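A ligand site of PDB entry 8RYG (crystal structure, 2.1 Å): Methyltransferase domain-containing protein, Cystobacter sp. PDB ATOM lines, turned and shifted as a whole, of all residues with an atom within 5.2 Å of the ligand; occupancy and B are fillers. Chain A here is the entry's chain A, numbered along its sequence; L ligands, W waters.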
ATOM      1  N   TYR A   6     -19.078 -12.347   1.902  1.00  0.00           N
ATOM      2  CA  TYR A   6     -17.956 -13.324   2.022  1.00  0.00           C
ATOM      3  C   TYR A   6     -16.694 -12.754   1.362  1.00  0.00           C
ATOM      4  O   TYR A   6     -15.610 -12.877   1.957  1.00  0.00           O
ATOM      5  CB  TYR A   6     -18.328 -14.655   1.381  1.00  0.00           C
ATOM      6  CG  TYR A   6     -19.573 -15.300   1.932  1.00  0.00           C
ATOM      7  CD1 TYR A   6     -19.576 -15.919   3.169  1.00  0.00           C
ATOM      8  CD2 TYR A   6     -20.757 -15.288   1.207  1.00  0.00           C
ATOM      9  CE1 TYR A   6     -20.720 -16.504   3.680  1.00  0.00           C
ATOM     10  CE2 TYR A   6     -21.909 -15.879   1.698  1.00  0.00           C
ATOM     11  CZ  TYR A   6     -21.895 -16.487   2.945  1.00  0.00           C
ATOM     12  OH  TYR A   6     -23.029 -17.062   3.430  1.00  0.00           O
ATOM     13  N   LEU A  14     -18.023 -16.546  10.415  1.00  0.00           N
ATOM     14  CA  LEU A  14     -18.984 -17.668  10.581  1.00  0.00           C
ATOM     15  C   LEU A  14     -18.271 -19.026  10.680  1.00  0.00           C
ATOM     16  O   LEU A  14     -18.952 -19.994  11.057  1.00  0.00           O
ATOM     17  CB  LEU A  14     -19.990 -17.636   9.421  1.00  0.00           C
ATOM     18  CG  LEU A  14     -20.974 -16.468   9.468  1.00  0.00           C
ATOM     19  CD1 LEU A  14     -21.574 -16.206   8.090  1.00  0.00           C
ATOM     20  CD2 LEU A  14     -22.068 -16.715  10.495  1.00  0.00           C
ATOM     21  N   VAL A  48     -21.037 -28.637  -1.022  1.00  0.00           N
ATOM     22  CA  VAL A  48     -21.772 -27.488  -1.625  1.00  0.00           C
ATOM     23  C   VAL A  48     -21.832 -26.352  -0.596  1.00  0.00           C
ATOM     24  O   VAL A  48     -22.530 -26.512   0.414  1.00  0.00           O
ATOM     25  CB  VAL A  48     -23.179 -27.898  -2.094  1.00  0.00           C
ATOM     26  CG1 VAL A  48     -23.900 -26.762  -2.783  1.00  0.00           C
ATOM     27  CG2 VAL A  48     -23.137 -29.129  -3.007  1.00  0.00           C
ATOM     28  N   GLY A  49     -21.132 -25.245  -0.850  1.00  0.00           N
ATOM     29  CA  GLY A  49     -20.805 -24.226   0.166  1.00  0.00           C
ATOM     30  C   GLY A  49     -19.574 -24.641   0.947  1.00  0.00           C
ATOM     31  O   GLY A  49     -19.615 -24.608   2.190  1.00  0.00           O
ATOM     32  N   SER A  50     -18.512 -25.024   0.232  1.00  0.00           N
ATOM     33  CA  SER A  50     -17.289 -25.677   0.745  1.00  0.00           C
ATOM     34  C   SER A  50     -16.401 -24.685   1.498  1.00  0.00           C
ATOM     35  O   SER A  50     -15.645 -25.137   2.388  1.00  0.00           O
ATOM     36  CB  SER A  50     -16.513 -26.306  -0.381  1.00  0.00           C
ATOM     37  OG  SER A  50     -16.038 -25.328  -1.285  1.00  0.00           O
ATOM     38  N   MET A  51     -16.471 -23.405   1.142  1.00  0.00           N
ATOM     39  CA  MET A  51     -15.455 -22.381   1.525  1.00  0.00           C
ATOM     40  C   MET A  51     -14.075 -22.921   1.122  1.00  0.00           C
ATOM     41  O   MET A  51     -13.980 -23.478   0.000  1.00  0.00           O
ATOM     42  CB  MET A  51     -15.519 -22.087   3.023  1.00  0.00           C
ATOM     43  CG  MET A  51     -16.925 -21.756   3.493  1.00  0.00           C
ATOM     44  SD  MET A  51     -17.019 -21.077   5.164  1.00  0.00           S
ATOM     45  CE  MET A  51     -16.269 -19.470   4.943  1.00  0.00           C
ATOM     46  N   VAL A  69     -17.544 -27.061  -3.828  1.00  0.00           N
ATOM     47  CA  VAL A  69     -18.301 -26.079  -4.665  1.00  0.00           C
ATOM     48  C   VAL A  69     -18.587 -24.842  -3.803  1.00  0.00           C
ATOM     49  O   VAL A  69     -19.192 -25.001  -2.731  1.00  0.00           O
ATOM     50  CB  VAL A  69     -19.597 -26.694  -5.239  1.00  0.00           C
ATOM     51  CG1 VAL A  69     -20.278 -25.749  -6.223  1.00  0.00           C
ATOM     52  CG2 VAL A  69     -19.325 -28.034  -5.914  1.00  0.00           C
ATOM     53  N   ASP A  70     -18.140 -23.665  -4.265  1.00  0.00           N
ATOM     54  CA  ASP A  70     -18.384 -22.363  -3.586  1.00  0.00           C
ATOM     55  C   ASP A  70     -18.291 -21.233  -4.616  1.00  0.00           C
ATOM     56  O   ASP A  70     -17.397 -21.245  -5.462  1.00  0.00           O
ATOM     57  CB  ASP A  70     -17.400 -22.163  -2.432  1.00  0.00           C
ATOM     58  CG  ASP A  70     -17.916 -21.246  -1.336  1.00  0.00           C
ATOM     59  OD1 ASP A  70     -18.048 -20.039  -1.604  1.00  0.00           O
ATOM     60  OD2 ASP A  70     -18.204 -21.735  -0.222  1.00  0.00           O
ATOM     61  N   PRO A  71     -19.228 -20.254  -4.611  1.00  0.00           N
ATOM     62  CA  PRO A  71     -19.146 -19.124  -5.528  1.00  0.00           C
ATOM     63  C   PRO A  71     -18.140 -18.015  -5.159  1.00  0.00           C
ATOM     64  O   PRO A  71     -17.997 -17.112  -5.940  1.00  0.00           O
ATOM     65  CB  PRO A  71     -20.570 -18.547  -5.503  1.00  0.00           C
ATOM     66  CG  PRO A  71     -21.100 -18.906  -4.124  1.00  0.00           C
ATOM     67  CD  PRO A  71     -20.444 -20.227  -3.779  1.00  0.00           C
ATOM     68  N   VAL A  72     -17.459 -18.108  -4.016  1.00  0.00           N
ATOM     69  CA  VAL A  72     -16.489 -17.079  -3.528  1.00  0.00           C
ATOM     70  C   VAL A  72     -15.100 -17.431  -4.066  1.00  0.00           C
ATOM     71  O   VAL A  72     -14.497 -18.415  -3.635  1.00  0.00           O
ATOM     72  CB  VAL A  72     -16.499 -16.959  -1.995  1.00  0.00           C
ATOM     73  CG1 VAL A  72     -15.552 -15.869  -1.504  1.00  0.00           C
ATOM     74  CG2 VAL A  72     -17.901 -16.703  -1.460  1.00  0.00           C
ATOM     75  N   TYR A  75     -12.140 -18.124  -1.561  1.00  0.00           N
ATOM     76  CA  TYR A  75     -12.326 -19.429  -0.863  1.00  0.00           C
ATOM     77  C   TYR A  75     -11.853 -20.578  -1.756  1.00  0.00           C
ATOM     78  O   TYR A  75     -11.221 -21.518  -1.244  1.00  0.00           O
ATOM     79  CB  TYR A  75     -13.797 -19.640  -0.461  1.00  0.00           C
ATOM     80  CG  TYR A  75     -14.318 -18.746   0.628  1.00  0.00           C
ATOM     81  CD1 TYR A  75     -13.475 -18.046   1.478  1.00  0.00           C
ATOM     82  CD2 TYR A  75     -15.689 -18.625   0.841  1.00  0.00           C
ATOM     83  CE1 TYR A  75     -13.974 -17.232   2.482  1.00  0.00           C
ATOM     84  CE2 TYR A  75     -16.204 -17.816   1.848  1.00  0.00           C
ATOM     85  CZ  TYR A  75     -15.339 -17.119   2.675  1.00  0.00           C
ATOM     86  OH  TYR A  75     -15.839 -16.314   3.652  1.00  0.00           O
ATOM     87  N   GLY A  98     -18.673 -21.846  -8.337  1.00  0.00           N
ATOM     88  CA  GLY A  98     -20.058 -21.768  -8.858  1.00  0.00           C
ATOM     89  C   GLY A  98     -21.082 -21.809  -7.726  1.00  0.00           C
ATOM     90  O   GLY A  98     -20.678 -22.008  -6.572  1.00  0.00           O
ATOM     91  N   GLY A  99     -22.359 -21.638  -8.068  1.00  0.00           N
ATOM     92  CA  GLY A  99     -23.496 -21.696  -7.119  1.00  0.00           C
ATOM     93  C   GLY A  99     -24.219 -23.024  -7.192  1.00  0.00           C
ATOM     94  O   GLY A  99     -24.207 -23.657  -8.275  1.00  0.00           O
ATOM     95  N   ALA A 100     -24.845 -23.437  -6.082  1.00  0.00           N
ATOM     96  CA  ALA A 100     -25.727 -24.636  -5.990  1.00  0.00           C
ATOM     97  C   ALA A 100     -26.864 -24.523  -7.007  1.00  0.00           C
ATOM     98  O   ALA A 100     -27.356 -25.582  -7.454  1.00  0.00           O
ATOM     99  CB  ALA A 100     -26.256 -24.793  -4.592  1.00  0.00           C
ATOM    100  N   GLU A 101     -27.264 -23.296  -7.360  1.00  0.00           N
ATOM    101  CA  GLU A 101     -28.314 -22.980  -8.362  1.00  0.00           C
ATOM    102  C   GLU A 101     -27.991 -23.659  -9.705  1.00  0.00           C
ATOM    103  O   GLU A 101     -28.945 -24.018 -10.407  1.00  0.00           O
ATOM    104  CB  GLU A 101     -28.455 -21.467  -8.541  1.00  0.00           C
ATOM    105  CG  GLU A 101     -29.077 -20.758  -7.337  1.00  0.00           C
ATOM    106  CD  GLU A 101     -28.129 -20.329  -6.232  1.00  0.00           C
ATOM    107  OE1 GLU A 101     -26.921 -20.677  -6.306  1.00  0.00           O
ATOM    108  OE2 GLU A 101     -28.589 -19.645  -5.296  1.00  0.00           O
ATOM    109  N   PHE A 125     -23.147 -26.962   7.394  1.00  0.00           N
ATOM    110  CA  PHE A 125     -23.192 -25.776   8.300  1.00  0.00           C
ATOM    111  C   PHE A 125     -24.184 -24.731   7.759  1.00  0.00           C
ATOM    112  O   PHE A 125     -23.875 -23.537   7.859  1.00  0.00           O
ATOM    113  CB  PHE A 125     -21.788 -25.194   8.461  1.00  0.00           C
ATOM    114  CG  PHE A 125     -21.502 -24.460   9.743  1.00  0.00           C
ATOM    115  CD1 PHE A 125     -22.507 -24.150  10.654  1.00  0.00           C
ATOM    116  CD2 PHE A 125     -20.201 -24.062  10.049  1.00  0.00           C
ATOM    117  CE1 PHE A 125     -22.215 -23.465  11.833  1.00  0.00           C
ATOM    118  CE2 PHE A 125     -19.918 -23.388  11.225  1.00  0.00           C
ATOM    119  CZ  PHE A 125     -20.926 -23.096  12.112  1.00  0.00           C
ATOM    120  N   ASN A 126     -25.301 -25.187   7.196  1.00  0.00           N
ATOM    121  CA  ASN A 126     -26.459 -24.356   6.768  1.00  0.00           C
ATOM    122  C   ASN A 126     -26.076 -23.444   5.592  1.00  0.00           C
ATOM    123  O   ASN A 126     -26.643 -22.340   5.515  1.00  0.00           O
ATOM    124  CB  ASN A 126     -27.031 -23.552   7.937  1.00  0.00           C
ATOM    125  CG  ASN A 126     -28.330 -22.852   7.599  1.00  0.00           C
ATOM    126  OD1 ASN A 126     -29.189 -23.435   6.941  1.00  0.00           O
ATOM    127  ND2 ASN A 126     -28.475 -21.605   8.008  1.00  0.00           N
ATOM    128  N   SER A 127     -25.204 -23.894   4.691  1.00  0.00           N
ATOM    129  CA  SER A 127     -24.873 -23.200   3.421  1.00  0.00           C
ATOM    130  C   SER A 127     -26.159 -22.975   2.618  1.00  0.00           C
ATOM    131  O   SER A 127     -26.312 -21.876   2.038  1.00  0.00           O
ATOM    132  CB  SER A 127     -23.846 -23.957   2.613  1.00  0.00           C
ATOM    133  OG  SER A 127     -24.382 -25.161   2.069  1.00  0.00           O
ATOM    134  N   ASN A 130     -28.203 -19.876   3.295  1.00  0.00           N
ATOM    135  CA  ASN A 130     -27.567 -18.584   2.911  1.00  0.00           C
ATOM    136  C   ASN A 130     -27.712 -18.343   1.408  1.00  0.00           C
ATOM    137  O   ASN A 130     -27.158 -17.344   0.913  1.00  0.00           O
ATOM    138  CB  ASN A 130     -26.109 -18.511   3.323  1.00  0.00           C
ATOM    139  CG  ASN A 130     -25.959 -18.428   4.825  1.00  0.00           C
ATOM    140  OD1 ASN A 130     -26.285 -19.378   5.540  1.00  0.00           O
ATOM    141  ND2 ASN A 130     -25.480 -17.293   5.321  1.00  0.00           N
ATOM    142  N   MET A 131     -28.427 -19.234   0.710  1.00  0.00           N
ATOM    143  CA  MET A 131     -28.558 -19.189  -0.756  1.00  0.00           C
ATOM    144  C   MET A 131     -29.741 -18.302  -1.134  1.00  0.00           C
ATOM    145  O   MET A 131     -30.785 -18.366  -0.443  1.00  0.00           O
ATOM    146  CB  MET A 131     -28.703 -20.599  -1.320  1.00  0.00           C
ATOM    147  CG  MET A 131     -27.566 -21.491  -0.862  1.00  0.00           C
ATOM    148  SD  MET A 131     -27.425 -23.057  -1.737  1.00  0.00           S
ATOM    149  CE  MET A 131     -25.885 -23.656  -1.024  1.00  0.00           C
ATOM    150  N   TYR A 153     -30.785 -26.139  10.397  1.00  0.00           N
ATOM    151  CA  TYR A 153     -31.239 -26.018  11.799  1.00  0.00           C
ATOM    152  C   TYR A 153     -32.736 -26.324  11.890  1.00  0.00           C
ATOM    153  O   TYR A 153     -33.444 -26.238  10.864  1.00  0.00           O
ATOM    154  CB  TYR A 153     -30.939 -24.605  12.318  1.00  0.00           C
ATOM    155  CG  TYR A 153     -29.492 -24.195  12.208  1.00  0.00           C
ATOM    156  CD1 TYR A 153     -28.546 -24.703  13.094  1.00  0.00           C
ATOM    157  CD2 TYR A 153     -29.069 -23.304  11.240  1.00  0.00           C
ATOM    158  CE1 TYR A 153     -27.214 -24.324  13.008  1.00  0.00           C
ATOM    159  CE2 TYR A 153     -27.742 -22.912  11.156  1.00  0.00           C
ATOM    160  CZ  TYR A 153     -26.810 -23.417  12.042  1.00  0.00           C
ATOM    161  OH  TYR A 153     -25.501 -23.040  11.964  1.00  0.00           O
ATOM    162  N   ARG A 163     -28.553 -20.315  17.263  1.00  0.00           N
ATOM    163  CA  ARG A 163     -28.141 -19.534  16.071  1.00  0.00           C
ATOM    164  C   ARG A 163     -27.870 -18.076  16.456  1.00  0.00           C
ATOM    165  O   ARG A 163     -26.876 -17.516  15.960  1.00  0.00           O
ATOM    166  CB  ARG A 163     -29.222 -19.609  14.990  1.00  0.00           C
ATOM    167  CG  ARG A 163     -29.436 -21.000  14.407  1.00  0.00           C
ATOM    168  CD  ARG A 163     -30.570 -20.972  13.398  1.00  0.00           C
ATOM    169  NE  ARG A 163     -30.177 -20.288  12.166  1.00  0.00           N
ATOM    170  CZ  ARG A 163     -31.010 -19.651  11.349  1.00  0.00           C
ATOM    171  NH1 ARG A 163     -32.298 -19.574  11.612  1.00  0.00           N
ATOM    172  NH2 ARG A 163     -30.530 -19.079  10.257  1.00  0.00           N
ATOM    173  N   TYR A 166     -24.626 -17.716  18.234  1.00  0.00           N
ATOM    174  CA  TYR A 166     -23.535 -17.973  17.256  1.00  0.00           C
ATOM    175  C   TYR A 166     -23.320 -16.720  16.402  1.00  0.00           C
ATOM    176  O   TYR A 166     -22.197 -16.196  16.371  1.00  0.00           O
ATOM    177  CB  TYR A 166     -23.882 -19.244  16.464  1.00  0.00           C
ATOM    178  CG  TYR A 166     -23.202 -19.444  15.139  1.00  0.00           C
ATOM    179  CD1 TYR A 166     -21.869 -19.142  14.930  1.00  0.00           C
ATOM    180  CD2 TYR A 166     -23.888 -20.026  14.084  1.00  0.00           C
ATOM    181  CE1 TYR A 166     -21.245 -19.356  13.710  1.00  0.00           C
ATOM    182  CE2 TYR A 166     -23.284 -20.260  12.857  1.00  0.00           C
ATOM    183  CZ  TYR A 166     -21.964 -19.914  12.670  1.00  0.00           C
ATOM    184  OH  TYR A 166     -21.370 -20.131  11.452  1.00  0.00           O
ATOM    185  N   TYR A 167     -24.381 -16.241  15.756  1.00  0.00           N
ATOM    186  CA  TYR A 167     -24.352 -15.090  14.803  1.00  0.00           C
ATOM    187  C   TYR A 167     -23.947 -13.795  15.546  1.00  0.00           C
ATOM    188  O   TYR A 167     -23.186 -13.017  14.962  1.00  0.00           O
ATOM    189  CB  TYR A 167     -25.691 -14.928  14.093  1.00  0.00           C
ATOM    190  CG  TYR A 167     -26.143 -16.121  13.272  1.00  0.00           C
ATOM    191  CD1 TYR A 167     -25.245 -17.029  12.748  1.00  0.00           C
ATOM    192  CD2 TYR A 167     -27.486 -16.312  13.000  1.00  0.00           C
ATOM    193  CE1 TYR A 167     -25.674 -18.106  11.989  1.00  0.00           C
ATOM    194  CE2 TYR A 167     -27.935 -17.382  12.248  1.00  0.00           C
ATOM    195  CZ  TYR A 167     -27.015 -18.283  11.728  1.00  0.00           C
ATOM    196  OH  TYR A 167     -27.454 -19.343  10.979  1.00  0.00           O
ATOM    197  N   PHE A 192     -25.268 -10.290   5.451  1.00  0.00           N
ATOM    198  CA  PHE A 192     -25.663 -11.563   6.102  1.00  0.00           C
ATOM    199  C   PHE A 192     -27.177 -11.752   5.965  1.00  0.00           C
ATOM    200  O   PHE A 192     -27.941 -10.823   6.303  1.00  0.00           O
ATOM    201  CB  PHE A 192     -25.227 -11.566   7.577  1.00  0.00           C
ATOM    202  CG  PHE A 192     -25.481 -12.851   8.316  1.00  0.00           C
ATOM    203  CD1 PHE A 192     -24.985 -14.062   7.841  1.00  0.00           C
ATOM    204  CD2 PHE A 192     -26.174 -12.856   9.518  1.00  0.00           C
ATOM    205  CE1 PHE A 192     -25.208 -15.240   8.534  1.00  0.00           C
ATOM    206  CE2 PHE A 192     -26.389 -14.033  10.218  1.00  0.00           C
ATOM    207  CZ  PHE A 192     -25.903 -15.227   9.723  1.00  0.00           C
ATOM    208  N   ALA A 194     -29.367 -15.411   6.543  1.00  0.00           N
ATOM    209  CA  ALA A 194     -29.273 -16.856   6.850  1.00  0.00           C
ATOM    210  C   ALA A 194     -30.644 -17.358   7.326  1.00  0.00           C
ATOM    211  O   ALA A 194     -31.137 -16.844   8.345  1.00  0.00           O
ATOM    212  CB  ALA A 194     -28.201 -17.097   7.892  1.00  0.00           C
HETATM  213  N1  LIG L   1     -22.539 -21.336   8.784  1.00  0.00           N
HETATM  214  C1  LIG L   1     -23.429 -20.141   8.569  1.00  0.00           C
HETATM  215  C2  LIG L   1     -23.432 -19.641   7.119  1.00  0.00           C
HETATM  216  C3  LIG L   1     -23.141 -20.690   6.057  1.00  0.00           C
HETATM  217  S1  LIG L   1     -22.686 -19.977   4.436  1.00  0.00           S
HETATM  218  C4  LIG L   1     -24.853 -20.491   9.010  1.00  0.00           C
HETATM  219  O1  LIG L   1     -25.004 -21.232   9.996  1.00  0.00           O
HETATM  220  O2  LIG L   1     -25.859 -20.077   8.429  1.00  0.00           O
HETATM  221  C5  LIG L   1     -21.328 -21.108   4.038  1.00  0.00           C
HETATM  222  C6  LIG L   1     -20.771 -21.093   2.628  1.00  0.00           C
HETATM  223  O3  LIG L   1     -21.863 -21.226   1.681  1.00  0.00           O
HETATM  224  C7  LIG L   1     -20.009 -19.823   2.232  1.00  0.00           C
HETATM  225  O4  LIG L   1     -18.723 -20.114   1.707  1.00  0.00           O
HETATM  226  C8  LIG L   1     -20.857 -19.235   1.088  1.00  0.00           C
HETATM  227  O5  LIG L   1     -20.107 -18.570   0.095  1.00  0.00           O
HETATM  228  C9  LIG L   1     -21.459 -20.514   0.536  1.00  0.00           C
HETATM  229  N2  LIG L   1     -22.580 -20.277  -0.368  1.00  0.00           N
HETATM  230  C10 LIG L   1     -23.439 -19.203  -0.354  1.00  0.00           C
HETATM  231  N3  LIG L   1     -24.310 -19.223  -1.328  1.00  0.00           N
HETATM  232  C11 LIG L   1     -23.986 -20.364  -2.053  1.00  0.00           C
HETATM  233  C12 LIG L   1     -24.537 -20.937  -3.207  1.00  0.00           C
HETATM  234  N4  LIG L   1     -25.549 -20.403  -3.883  1.00  0.00           N
HETATM  235  N5  LIG L   1     -23.974 -22.073  -3.674  1.00  0.00           N
HETATM  236  C13 LIG L   1     -22.938 -22.600  -2.995  1.00  0.00           C
HETATM  237  N6  LIG L   1     -22.348 -22.154  -1.895  1.00  0.00           N
HETATM  238  C14 LIG L   1     -22.917 -21.019  -1.465  1.00  0.00           C
HETATM  239  O   HOH W   1     -20.745 -24.320   4.584  1.00  0.00           O
HETATM  240  O   HOH W   2     -27.161 -18.057  -3.539  1.00  0.00           O
HETATM  241  O   HOH W   3     -20.026 -20.785   8.270  1.00  0.00           O
HETATM  242  O   HOH W   4     -25.515 -16.620  -1.730  1.00  0.00           O
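A nitrogen (N4) of the ligand lies within hydrogen-bond range of the side-chain carboxylate of Glu 101, 2.8 Å away.
OH of Tyr 167 lies within hydrogen-bond range of O2 of the ligand (3.1 Å).
An oxygen (O2) of the ligand sits close to the side-chain amide oxygen of Asn 130 (3.0 Å).
ND2 of Asn 126 sits at hydrogen-bond distance from O2 of the ligand.
O4 of the ligand sits at hydrogen-bond distance from OD2 of Asp 70, at 2.6 Å.
The backbone carbonyl oxygen of Phe 125 is in hydrogen-bond range of a nitrogen (N1) of the ligand (2.7 Å).
A sulfur (S1) of the ligand lies close to the side-chain hydroxyl (OH) of Tyr 6 (3.1 Å).
N of Gly 49 lies close to N6 of the ligand (3.5 Å).
An oxygen (O1) of the ligand sits at hydrogen-bond distance from the side-chain hydroxyl (OH) of Tyr 153.
N of Ala 100 lies within hydrogen-bond range of N5 of the ligand, at 2.9 Å.
N1 of the ligand sits at hydrogen-bond distance from OH of Tyr 166, 3.2 Å away.
The side-chain hydroxyl of Ser 127 is in hydrogen-bond range of the backbone carbonyl oxygen of Val 48.
The backbone NH of Gly 49 lies within hydrogen-bond range of the backbone carbonyl oxygen of Val 69 (2.7 Å).
The backbone NH of Gly 98 is in hydrogen-bond range of the backbone carbonyl oxygen of Asp 70 (3.2 Å).
OD1 of Asp 70 lies within hydrogen-bond range of N of Val 72.
The backbone carbonyl oxygen of Asn 126 sits close to the side-chain amide oxygen of Asn 130 (3.0 Å).
The side-chain hydroxyl of Tyr 6 sits at hydrogen-bond distance from the side-chain amide nitrogen of Asn 130, at 3.1 Å.
The backbone NH (N) of Met 51 lies within hydrogen-bond range of the side-chain carboxylate (OD2) of Asp 70, 2.8 Å away.
The guanidinium group (NE) of Arg 163 sits at hydrogen-bond distance from the side-chain hydroxyl (OH) of Tyr 167 (3.1 Å).
Met 51 touches the ligand (CG to O4, 3.0 Å).
Pro 71 touches the ligand (CD to N6, 3.3 Å).
CG2 of Val 72 touches O5 of the ligand (3.3 Å).
CE2 of Tyr 75 touches O4 of the ligand (3.4 Å).
Gly 99 touches the ligand.
Ser 127 touches the ligand (CB to O3, 3.5 Å).
Met 131 touches the ligand.
Ala 194 touches the ligand (CB to O2, 3.8 Å).
Of the 26 residues printed, 19 come within 4 Å of the ligand.
Water W3 lies within hydrogen-bond range of a nitrogen (N1) of the ligand and the backbone carbonyl oxygen of Leu 14.
Water W2 lies within hydrogen-bond range of the side-chain carboxylate of Glu 101 (2.8 Å) and a nitrogen (N4) of the ligand (2.9 Å).
Water W4 bridges a nitrogen (N3) of the ligand (2.9 Å) and the backbone carbonyl oxygen (O) of Asn 130 (3.2 Å).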
